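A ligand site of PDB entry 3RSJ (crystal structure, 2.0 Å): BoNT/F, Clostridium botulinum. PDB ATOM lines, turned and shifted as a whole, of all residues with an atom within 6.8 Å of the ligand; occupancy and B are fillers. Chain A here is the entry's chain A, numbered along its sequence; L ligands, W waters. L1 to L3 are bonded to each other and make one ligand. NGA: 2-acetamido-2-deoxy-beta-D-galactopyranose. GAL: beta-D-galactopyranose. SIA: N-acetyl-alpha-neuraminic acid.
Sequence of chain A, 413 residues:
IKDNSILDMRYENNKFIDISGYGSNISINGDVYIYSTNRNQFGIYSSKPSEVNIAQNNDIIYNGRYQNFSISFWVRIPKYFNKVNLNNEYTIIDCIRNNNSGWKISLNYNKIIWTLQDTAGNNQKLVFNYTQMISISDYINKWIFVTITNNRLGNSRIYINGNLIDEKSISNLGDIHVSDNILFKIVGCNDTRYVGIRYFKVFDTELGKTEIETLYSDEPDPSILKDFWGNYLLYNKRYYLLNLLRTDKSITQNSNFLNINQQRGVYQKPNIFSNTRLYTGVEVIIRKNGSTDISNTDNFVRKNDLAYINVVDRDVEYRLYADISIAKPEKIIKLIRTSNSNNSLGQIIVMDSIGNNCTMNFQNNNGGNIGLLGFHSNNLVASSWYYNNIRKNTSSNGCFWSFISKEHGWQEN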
ATOM      1  N   LEU A 245     -18.866   9.881  32.035  1.00  0.00           N
ATOM      2  CA  LEU A 245     -19.316   9.902  30.644  1.00  0.00           C
ATOM      3  C   LEU A 245     -20.728   9.301  30.632  1.00  0.00           C
ATOM      4  O   LEU A 245     -21.691   9.940  30.183  1.00  0.00           O
ATOM      5  CB  LEU A 245     -18.387   9.102  29.735  1.00  0.00           C
ATOM      6  CG  LEU A 245     -18.374   9.541  28.254  1.00  0.00           C
ATOM      7  CD1 LEU A 245     -17.480   8.624  27.445  1.00  0.00           C
ATOM      8  CD2 LEU A 245     -19.769   9.542  27.693  1.00  0.00           C
ATOM      9  N   ARG A 246     -20.867   8.078  31.135  1.00  0.00           N
ATOM     10  CA  ARG A 246     -22.164   7.411  31.197  1.00  0.00           C
ATOM     11  C   ARG A 246     -22.752   7.540  32.613  1.00  0.00           C
ATOM     12  O   ARG A 246     -22.829   6.549  33.356  1.00  0.00           O
ATOM     13  CB  ARG A 246     -22.032   5.939  30.835  1.00  0.00           C
ATOM     14  CG  ARG A 246     -21.809   5.656  29.357  1.00  0.00           C
ATOM     15  CD  ARG A 246     -21.829   4.163  29.109  1.00  0.00           C
ATOM     16  NE  ARG A 246     -21.714   3.805  27.700  1.00  0.00           N
ATOM     17  CZ  ARG A 246     -21.671   2.546  27.265  1.00  0.00           C
ATOM     18  NH1 ARG A 246     -21.742   1.545  28.144  1.00  0.00           N
ATOM     19  NH2 ARG A 246     -21.569   2.279  25.977  1.00  0.00           N
ATOM     20  N   LYS A 328      -5.527  -6.978  23.216  1.00  0.00           N
ATOM     21  CA  LYS A 328      -6.205  -5.735  22.843  1.00  0.00           C
ATOM     22  C   LYS A 328      -5.921  -4.630  23.849  1.00  0.00           C
ATOM     23  O   LYS A 328      -5.632  -4.901  25.022  1.00  0.00           O
ATOM     24  CB  LYS A 328      -7.706  -5.996  22.735  1.00  0.00           C
ATOM     25  CG  LYS A 328      -8.092  -6.836  21.531  1.00  0.00           C
ATOM     26  CD  LYS A 328      -9.427  -7.539  21.722  1.00  0.00           C
ATOM     27  CE  LYS A 328      -9.279  -8.756  22.641  1.00  0.00           C
ATOM     28  NZ  LYS A 328     -10.535  -9.556  22.740  1.00  0.00           N
ATOM     29  N   PRO A 329      -5.987  -3.360  23.419  1.00  0.00           N
ATOM     30  CA  PRO A 329      -5.729  -2.238  24.326  1.00  0.00           C
ATOM     31  C   PRO A 329      -6.744  -2.148  25.465  1.00  0.00           C
ATOM     32  O   PRO A 329      -6.473  -1.518  26.497  1.00  0.00           O
ATOM     33  CB  PRO A 329      -5.762  -1.028  23.391  1.00  0.00           C
ATOM     34  CG  PRO A 329      -6.637  -1.459  22.282  1.00  0.00           C
ATOM     35  CD  PRO A 329      -6.237  -2.880  22.046  1.00  0.00           C
ATOM     36  N   GLU A 330      -7.902  -2.769  25.288  1.00  0.00           N
ATOM     37  CA  GLU A 330      -8.917  -2.779  26.330  1.00  0.00           C
ATOM     38  C   GLU A 330      -8.832  -4.083  27.092  1.00  0.00           C
ATOM     39  O   GLU A 330      -9.268  -5.129  26.618  1.00  0.00           O
ATOM     40  CB  GLU A 330     -10.320  -2.612  25.758  1.00  0.00           C
ATOM     41  CG  GLU A 330     -10.586  -1.265  25.129  1.00  0.00           C
ATOM     42  CD  GLU A 330     -10.044  -1.167  23.723  1.00  0.00           C
ATOM     43  OE1 GLU A 330     -10.148  -0.080  23.127  1.00  0.00           O
ATOM     44  OE2 GLU A 330      -9.501  -2.182  23.218  1.00  0.00           O
ATOM     45  N   GLY A 374     -11.717   2.587  32.610  1.00  0.00           N
ATOM     46  CA  GLY A 374     -12.780   3.166  31.806  1.00  0.00           C
ATOM     47  C   GLY A 374     -13.727   2.026  31.456  1.00  0.00           C
ATOM     48  O   GLY A 374     -13.972   1.149  32.289  1.00  0.00           O
ATOM     49  N   PHE A 375     -14.251   2.029  30.242  1.00  0.00           N
ATOM     50  CA  PHE A 375     -15.151   0.987  29.788  1.00  0.00           C
ATOM     51  C   PHE A 375     -15.042   0.913  28.268  1.00  0.00           C
ATOM     52  O   PHE A 375     -14.552   1.847  27.632  1.00  0.00           O
ATOM     53  CB  PHE A 375     -16.589   1.286  30.232  1.00  0.00           C
ATOM     54  CG  PHE A 375     -17.218   2.490  29.582  1.00  0.00           C
ATOM     55  CD1 PHE A 375     -17.838   2.379  28.330  1.00  0.00           C
ATOM     56  CD2 PHE A 375     -17.194   3.728  30.204  1.00  0.00           C
ATOM     57  CE1 PHE A 375     -18.433   3.490  27.727  1.00  0.00           C
ATOM     58  CE2 PHE A 375     -17.801   4.842  29.608  1.00  0.00           C
ATOM     59  CZ  PHE A 375     -18.414   4.724  28.373  1.00  0.00           C
ATOM     60  N   HIS A 376     -15.453  -0.200  27.680  1.00  0.00           N
ATOM     61  CA  HIS A 376     -15.367  -0.334  26.237  1.00  0.00           C
ATOM     62  C   HIS A 376     -16.711  -0.715  25.637  1.00  0.00           C
ATOM     63  O   HIS A 376     -17.362   0.116  25.005  1.00  0.00           O
ATOM     64  CB  HIS A 376     -14.307  -1.352  25.820  1.00  0.00           C
ATOM     65  CG  HIS A 376     -14.194  -1.530  24.344  1.00  0.00           C
ATOM     66  ND1 HIS A 376     -13.881  -0.506  23.481  1.00  0.00           N
ATOM     67  CD2 HIS A 376     -14.295  -2.643  23.577  1.00  0.00           C
ATOM     68  CE1 HIS A 376     -13.796  -0.966  22.249  1.00  0.00           C
ATOM     69  NE2 HIS A 376     -14.039  -2.261  22.275  1.00  0.00           N
ATOM     70  N   SER A 377     -17.111  -1.965  25.809  1.00  0.00           N
ATOM     71  CA  SER A 377     -18.405  -2.374  25.281  1.00  0.00           C
ATOM     72  C   SER A 377     -19.353  -2.040  26.414  1.00  0.00           C
ATOM     73  O   SER A 377     -19.725  -0.890  26.603  1.00  0.00           O
ATOM     74  CB  SER A 377     -18.427  -3.878  24.993  1.00  0.00           C
ATOM     75  OG  SER A 377     -19.677  -4.264  24.457  1.00  0.00           O
ATOM     76  N   ASN A 379     -18.505  -3.263  29.529  1.00  0.00           N
ATOM     77  CA  ASN A 379     -17.714  -3.601  30.706  1.00  0.00           C
ATOM     78  C   ASN A 379     -16.612  -2.601  31.018  1.00  0.00           C
ATOM     79  O   ASN A 379     -16.161  -1.853  30.142  1.00  0.00           O
ATOM     80  CB  ASN A 379     -17.071  -4.985  30.539  1.00  0.00           C
ATOM     81  CG  ASN A 379     -18.001  -6.005  29.919  1.00  0.00           C
ATOM     82  OD1 ASN A 379     -19.152  -6.147  30.326  1.00  0.00           O
ATOM     83  ND2 ASN A 379     -17.511  -6.733  28.921  1.00  0.00           N
ATOM     84  N   VAL A 381     -12.908  -1.494  31.765  1.00  0.00           N
ATOM     85  CA  VAL A 381     -11.633  -1.953  31.218  1.00  0.00           C
ATOM     86  C   VAL A 381     -10.541  -0.963  31.577  1.00  0.00           C
ATOM     87  O   VAL A 381     -10.815   0.159  31.984  1.00  0.00           O
ATOM     88  CB  VAL A 381     -11.681  -2.039  29.676  1.00  0.00           C
ATOM     89  CG1 VAL A 381     -12.864  -2.868  29.207  1.00  0.00           C
ATOM     90  CG2 VAL A 381     -11.736  -0.626  29.073  1.00  0.00           C
ATOM     91  N   ALA A 382      -9.303  -1.405  31.445  1.00  0.00           N
ATOM     92  CA  ALA A 382      -8.160  -0.537  31.676  1.00  0.00           C
ATOM     93  C   ALA A 382      -7.664  -0.380  30.247  1.00  0.00           C
ATOM     94  O   ALA A 382      -7.251  -1.358  29.625  1.00  0.00           O
ATOM     95  CB  ALA A 382      -7.131  -1.228  32.535  1.00  0.00           C
ATOM     96  N   SER A 383      -7.707   0.832  29.709  1.00  0.00           N
ATOM     97  CA  SER A 383      -7.270   1.014  28.340  1.00  0.00           C
ATOM     98  C   SER A 383      -6.252   2.112  28.141  1.00  0.00           C
ATOM     99  O   SER A 383      -6.373   3.210  28.698  1.00  0.00           O
ATOM    100  CB  SER A 383      -8.475   1.282  27.447  1.00  0.00           C
ATOM    101  OG  SER A 383      -8.057   1.377  26.104  1.00  0.00           O
ATOM    102  N   SER A 384      -5.239   1.825  27.324  1.00  0.00           N
ATOM    103  CA  SER A 384      -4.197   2.779  27.033  1.00  0.00           C
ATOM    104  C   SER A 384      -4.703   3.761  25.986  1.00  0.00           C
ATOM    105  O   SER A 384      -4.035   4.747  25.668  1.00  0.00           O
ATOM    106  CB  SER A 384      -2.928   2.077  26.526  1.00  0.00           C
ATOM    107  OG  SER A 384      -3.218   1.256  25.410  1.00  0.00           O
ATOM    108  N   TRP A 385      -5.901   3.500  25.465  1.00  0.00           N
ATOM    109  CA  TRP A 385      -6.491   4.372  24.460  1.00  0.00           C
ATOM    110  C   TRP A 385      -6.726   5.776  24.998  1.00  0.00           C
ATOM    111  O   TRP A 385      -6.613   6.752  24.280  1.00  0.00           O
ATOM    112  CB  TRP A 385      -7.827   3.793  23.975  1.00  0.00           C
ATOM    113  CG  TRP A 385      -8.553   4.663  22.967  1.00  0.00           C
ATOM    114  CD1 TRP A 385      -8.338   4.709  21.615  1.00  0.00           C
ATOM    115  CD2 TRP A 385      -9.583   5.619  23.246  1.00  0.00           C
ATOM    116  NE1 TRP A 385      -9.175   5.633  21.036  1.00  0.00           N
ATOM    117  CE2 TRP A 385      -9.952   6.202  22.008  1.00  0.00           C
ATOM    118  CE3 TRP A 385     -10.228   6.040  24.411  1.00  0.00           C
ATOM    119  CZ2 TRP A 385     -10.940   7.186  21.903  1.00  0.00           C
ATOM    120  CZ3 TRP A 385     -11.225   7.019  24.307  1.00  0.00           C
ATOM    121  CH2 TRP A 385     -11.563   7.583  23.059  1.00  0.00           C
ATOM    122  N   TYR A 386      -7.051   5.861  26.294  1.00  0.00           N
ATOM    123  CA  TYR A 386      -7.338   7.151  26.918  1.00  0.00           C
ATOM    124  C   TYR A 386      -6.183   8.136  26.975  1.00  0.00           C
ATOM    125  O   TYR A 386      -6.395   9.341  26.945  1.00  0.00           O
ATOM    126  CB  TYR A 386      -7.899   6.937  28.336  1.00  0.00           C
ATOM    127  CG  TYR A 386      -9.235   6.249  28.369  1.00  0.00           C
ATOM    128  CD1 TYR A 386      -9.360   4.937  28.823  1.00  0.00           C
ATOM    129  CD2 TYR A 386     -10.386   6.900  27.922  1.00  0.00           C
ATOM    130  CE1 TYR A 386     -10.585   4.287  28.826  1.00  0.00           C
ATOM    131  CE2 TYR A 386     -11.630   6.265  27.929  1.00  0.00           C
ATOM    132  CZ  TYR A 386     -11.721   4.955  28.382  1.00  0.00           C
ATOM    133  OH  TYR A 386     -12.940   4.313  28.375  1.00  0.00           O
ATOM    134  N   ASN A 389      -6.523  10.274  24.039  1.00  0.00           N
ATOM    135  CA  ASN A 389      -7.905  10.522  23.627  1.00  0.00           C
ATOM    136  C   ASN A 389      -8.795  11.088  24.728  1.00  0.00           C
ATOM    137  O   ASN A 389      -9.927  10.631  24.916  1.00  0.00           O
ATOM    138  CB  ASN A 389      -8.518   9.240  23.079  1.00  0.00           C
ATOM    139  CG  ASN A 389      -7.841   8.782  21.799  1.00  0.00           C
ATOM    140  OD1 ASN A 389      -7.870   9.495  20.800  1.00  0.00           O
ATOM    141  ND2 ASN A 389      -7.243   7.598  21.819  1.00  0.00           N
ATOM    142  N   ARG A 391     -10.823  14.350  26.090  1.00  0.00           N
ATOM    143  CA  ARG A 391     -11.352  15.637  25.663  1.00  0.00           C
ATOM    144  C   ARG A 391     -10.837  16.679  26.636  1.00  0.00           C
ATOM    145  O   ARG A 391     -10.903  16.495  27.846  1.00  0.00           O
ATOM    146  CB  ARG A 391     -12.878  15.640  25.657  1.00  0.00           C
ATOM    147  CG  ARG A 391     -13.549  14.797  24.573  1.00  0.00           C
ATOM    148  CD  ARG A 391     -13.452  13.313  24.886  1.00  0.00           C
ATOM    149  NE  ARG A 391     -14.346  12.506  24.055  1.00  0.00           N
ATOM    150  CZ  ARG A 391     -14.481  11.190  24.180  1.00  0.00           C
ATOM    151  NH1 ARG A 391     -13.779  10.529  25.084  1.00  0.00           N
ATOM    152  NH2 ARG A 391     -15.317  10.528  23.395  1.00  0.00           N
ATOM    153  N   ASN A 397     -15.590  12.177  29.877  1.00  0.00           N
ATOM    154  CA  ASN A 397     -14.548  11.273  29.428  1.00  0.00           C
ATOM    155  C   ASN A 397     -14.781   9.924  30.124  1.00  0.00           C
ATOM    156  O   ASN A 397     -14.907   9.860  31.347  1.00  0.00           O
ATOM    157  CB  ASN A 397     -13.157  11.819  29.803  1.00  0.00           C
ATOM    158  CG  ASN A 397     -12.697  12.935  28.887  1.00  0.00           C
ATOM    159  OD1 ASN A 397     -12.505  12.741  27.678  1.00  0.00           O
ATOM    160  ND2 ASN A 397     -12.511  14.124  29.452  1.00  0.00           N
ATOM    161  N   GLY A 398     -14.840   8.854  29.337  1.00  0.00           N
ATOM    162  CA  GLY A 398     -15.078   7.528  29.880  1.00  0.00           C
ATOM    163  C   GLY A 398     -14.136   7.116  30.993  1.00  0.00           C
ATOM    164  O   GLY A 398     -14.458   6.211  31.763  1.00  0.00           O
ATOM    165  N   CYS A 399     -12.973   7.766  31.087  1.00  0.00           N
ATOM    166  CA  CYS A 399     -11.996   7.434  32.117  1.00  0.00           C
ATOM    167  C   CYS A 399     -12.019   8.387  33.323  1.00  0.00           C
ATOM    168  O   CYS A 399     -11.067   8.438  34.096  1.00  0.00           O
ATOM    169  CB  CYS A 399     -10.589   7.410  31.521  1.00  0.00           C
ATOM    170  SG  CYS A 399     -10.064   8.980  30.796  1.00  0.00           S
HETATM  171  C1  NGA L   1     -10.908   1.975  17.643  1.00  0.00           C
HETATM  172  C2  NGA L   1     -12.140   1.764  18.551  1.00  0.00           C
HETATM  173  C3  NGA L   1     -11.911   2.342  19.968  1.00  0.00           C
HETATM  174  C4  NGA L   1     -10.655   1.649  20.504  1.00  0.00           C
HETATM  175  C5  NGA L   1      -9.438   1.839  19.580  1.00  0.00           C
HETATM  176  C6  NGA L   1      -8.191   1.134  20.091  1.00  0.00           C
HETATM  177  C7  NGA L   1     -14.335   1.738  17.448  1.00  0.00           C
HETATM  178  C8  NGA L   1     -15.485   1.357  18.262  1.00  0.00           C
HETATM  179  N2  NGA L   1     -13.330   2.395  18.016  1.00  0.00           N
HETATM  180  O1  NGA L   1     -11.130   1.425  16.343  1.00  0.00           O
HETATM  181  O3  NGA L   1     -13.031   2.105  20.791  1.00  0.00           O
HETATM  182  O4  NGA L   1     -10.991   0.280  20.628  1.00  0.00           O
HETATM  183  O5  NGA L   1      -9.751   1.346  18.252  1.00  0.00           O
HETATM  184  O6  NGA L   1      -8.361  -0.270  20.021  1.00  0.00           O
HETATM  185  O7  NGA L   1     -14.338   1.428  16.278  1.00  0.00           O
HETATM  186  C1  GAL L   2     -13.076   2.981  21.910  1.00  0.00           C
HETATM  187  C2  GAL L   2     -14.550   3.225  22.319  1.00  0.00           C
HETATM  188  C3  GAL L   2     -14.564   4.150  23.555  1.00  0.00           C
HETATM  189  C4  GAL L   2     -13.764   3.486  24.678  1.00  0.00           C
HETATM  190  C5  GAL L   2     -12.347   3.216  24.197  1.00  0.00           C
HETATM  191  C6  GAL L   2     -11.580   2.522  25.308  1.00  0.00           C
HETATM  192  O2  GAL L   2     -15.283   3.830  21.270  1.00  0.00           O
HETATM  193  O3  GAL L   2     -15.897   4.342  24.034  1.00  0.00           O
HETATM  194  O4  GAL L   2     -14.407   2.275  25.068  1.00  0.00           O
HETATM  195  O5  GAL L   2     -12.377   2.399  23.020  1.00  0.00           O
HETATM  196  O6  GAL L   2     -10.342   2.065  24.813  1.00  0.00           O
HETATM  197  C1  SIA L   3     -15.730   6.595  24.478  1.00  0.00           C
HETATM  198  C2  SIA L   3     -16.524   5.667  23.797  1.00  0.00           C
HETATM  199  C3  SIA L   3     -17.888   5.585  24.466  1.00  0.00           C
HETATM  200  C4  SIA L   3     -18.604   6.920  24.141  1.00  0.00           C
HETATM  201  C5  SIA L   3     -18.741   7.083  22.626  1.00  0.00           C
HETATM  202  C6  SIA L   3     -17.320   7.131  21.988  1.00  0.00           C
HETATM  203  C7  SIA L   3     -17.312   7.293  20.447  1.00  0.00           C
HETATM  204  C8  SIA L   3     -15.900   7.347  19.851  1.00  0.00           C
HETATM  205  C9  SIA L   3     -15.824   7.830  18.400  1.00  0.00           C
HETATM  206  C10 SIA L   3     -20.676   8.349  21.704  1.00  0.00           C
HETATM  207  C11 SIA L   3     -21.289   9.698  21.497  1.00  0.00           C
HETATM  208  N5  SIA L   3     -19.485   8.330  22.343  1.00  0.00           N
HETATM  209  O1A SIA L   3     -15.599   6.472  25.694  1.00  0.00           O
HETATM  210  O1B SIA L   3     -15.159   7.520  23.886  1.00  0.00           O
HETATM  211  O4  SIA L   3     -19.902   6.895  24.703  1.00  0.00           O
HETATM  212  O6  SIA L   3     -16.598   5.906  22.340  1.00  0.00           O
HETATM  213  O7  SIA L   3     -17.945   6.183  19.836  1.00  0.00           O
HETATM  214  O8  SIA L   3     -15.068   8.247  20.598  1.00  0.00           O
HETATM  215  O9  SIA L   3     -14.652   7.266  17.739  1.00  0.00           O
HETATM  216  O10 SIA L   3     -21.251   7.349  21.287  1.00  0.00           O
HETATM  217  O   HOH W   1     -14.093   8.667  26.792  1.00  0.00           O
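ND1 of His 376 sits close to O4 of GAL L2 (3.2 Å). OG of Ser 383 is in hydrogen-bond range of O6 of GAL L2, at 2.7 Å. OE1 of Glu 330 is in hydrogen-bond range of O4 of NGA L1 (2.7 Å). The backbone carbonyl oxygen (O) of Phe 375 lies within hydrogen-bond range of an oxygen (O4) of GAL L2, 2.6 Å away. NH2 of Arg 391 is in salt-bridge range of O1B of SIA L3, at 3.1 Å.
Merely in contact with the ligand: Leu 245, Pro 329, Trp 385 and Tyr 386. Hydrophobic or aromatic side chains that line the ligand: Leu 245, Pro 329, Phe 375, His 376, Trp 385 and Tyr 386. Nine residues have an atom within 4 Å of the ligand: Leu 245, Pro 329, Glu 330, Phe 375, His 376, Ser 383, Trp 385, Tyr 386 and Arg 391. Along chain A the residues within 4 Å of the ligand span positions 245 to 391.
OG of Ser 383 sits close to N of Trp 385, 3.1 Å away. The backbone carbonyl oxygen (O) of Phe 375 is in hydrogen-bond range of the side-chain hydroxyl (OH) of Tyr 386, at 3.0 Å. OD1 of Asn 397 lies within hydrogen-bond range of N of Arg 391 (2.8 Å). The backbone carbonyl oxygen (O) of Pro 329 sits close to the side-chain hydroxyl (OG) of Ser 383. O of Trp 385 is in hydrogen-bond range of ND2 of Asn 389.
Water W1 lies within hydrogen-bond range of the guanidinium group (NH1) of Arg 391 (2.5 Å), the backbone NH (N) of Gly 398 (2.7 Å) and an oxygen (O1A) of SIA L3 (2.9 Å).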
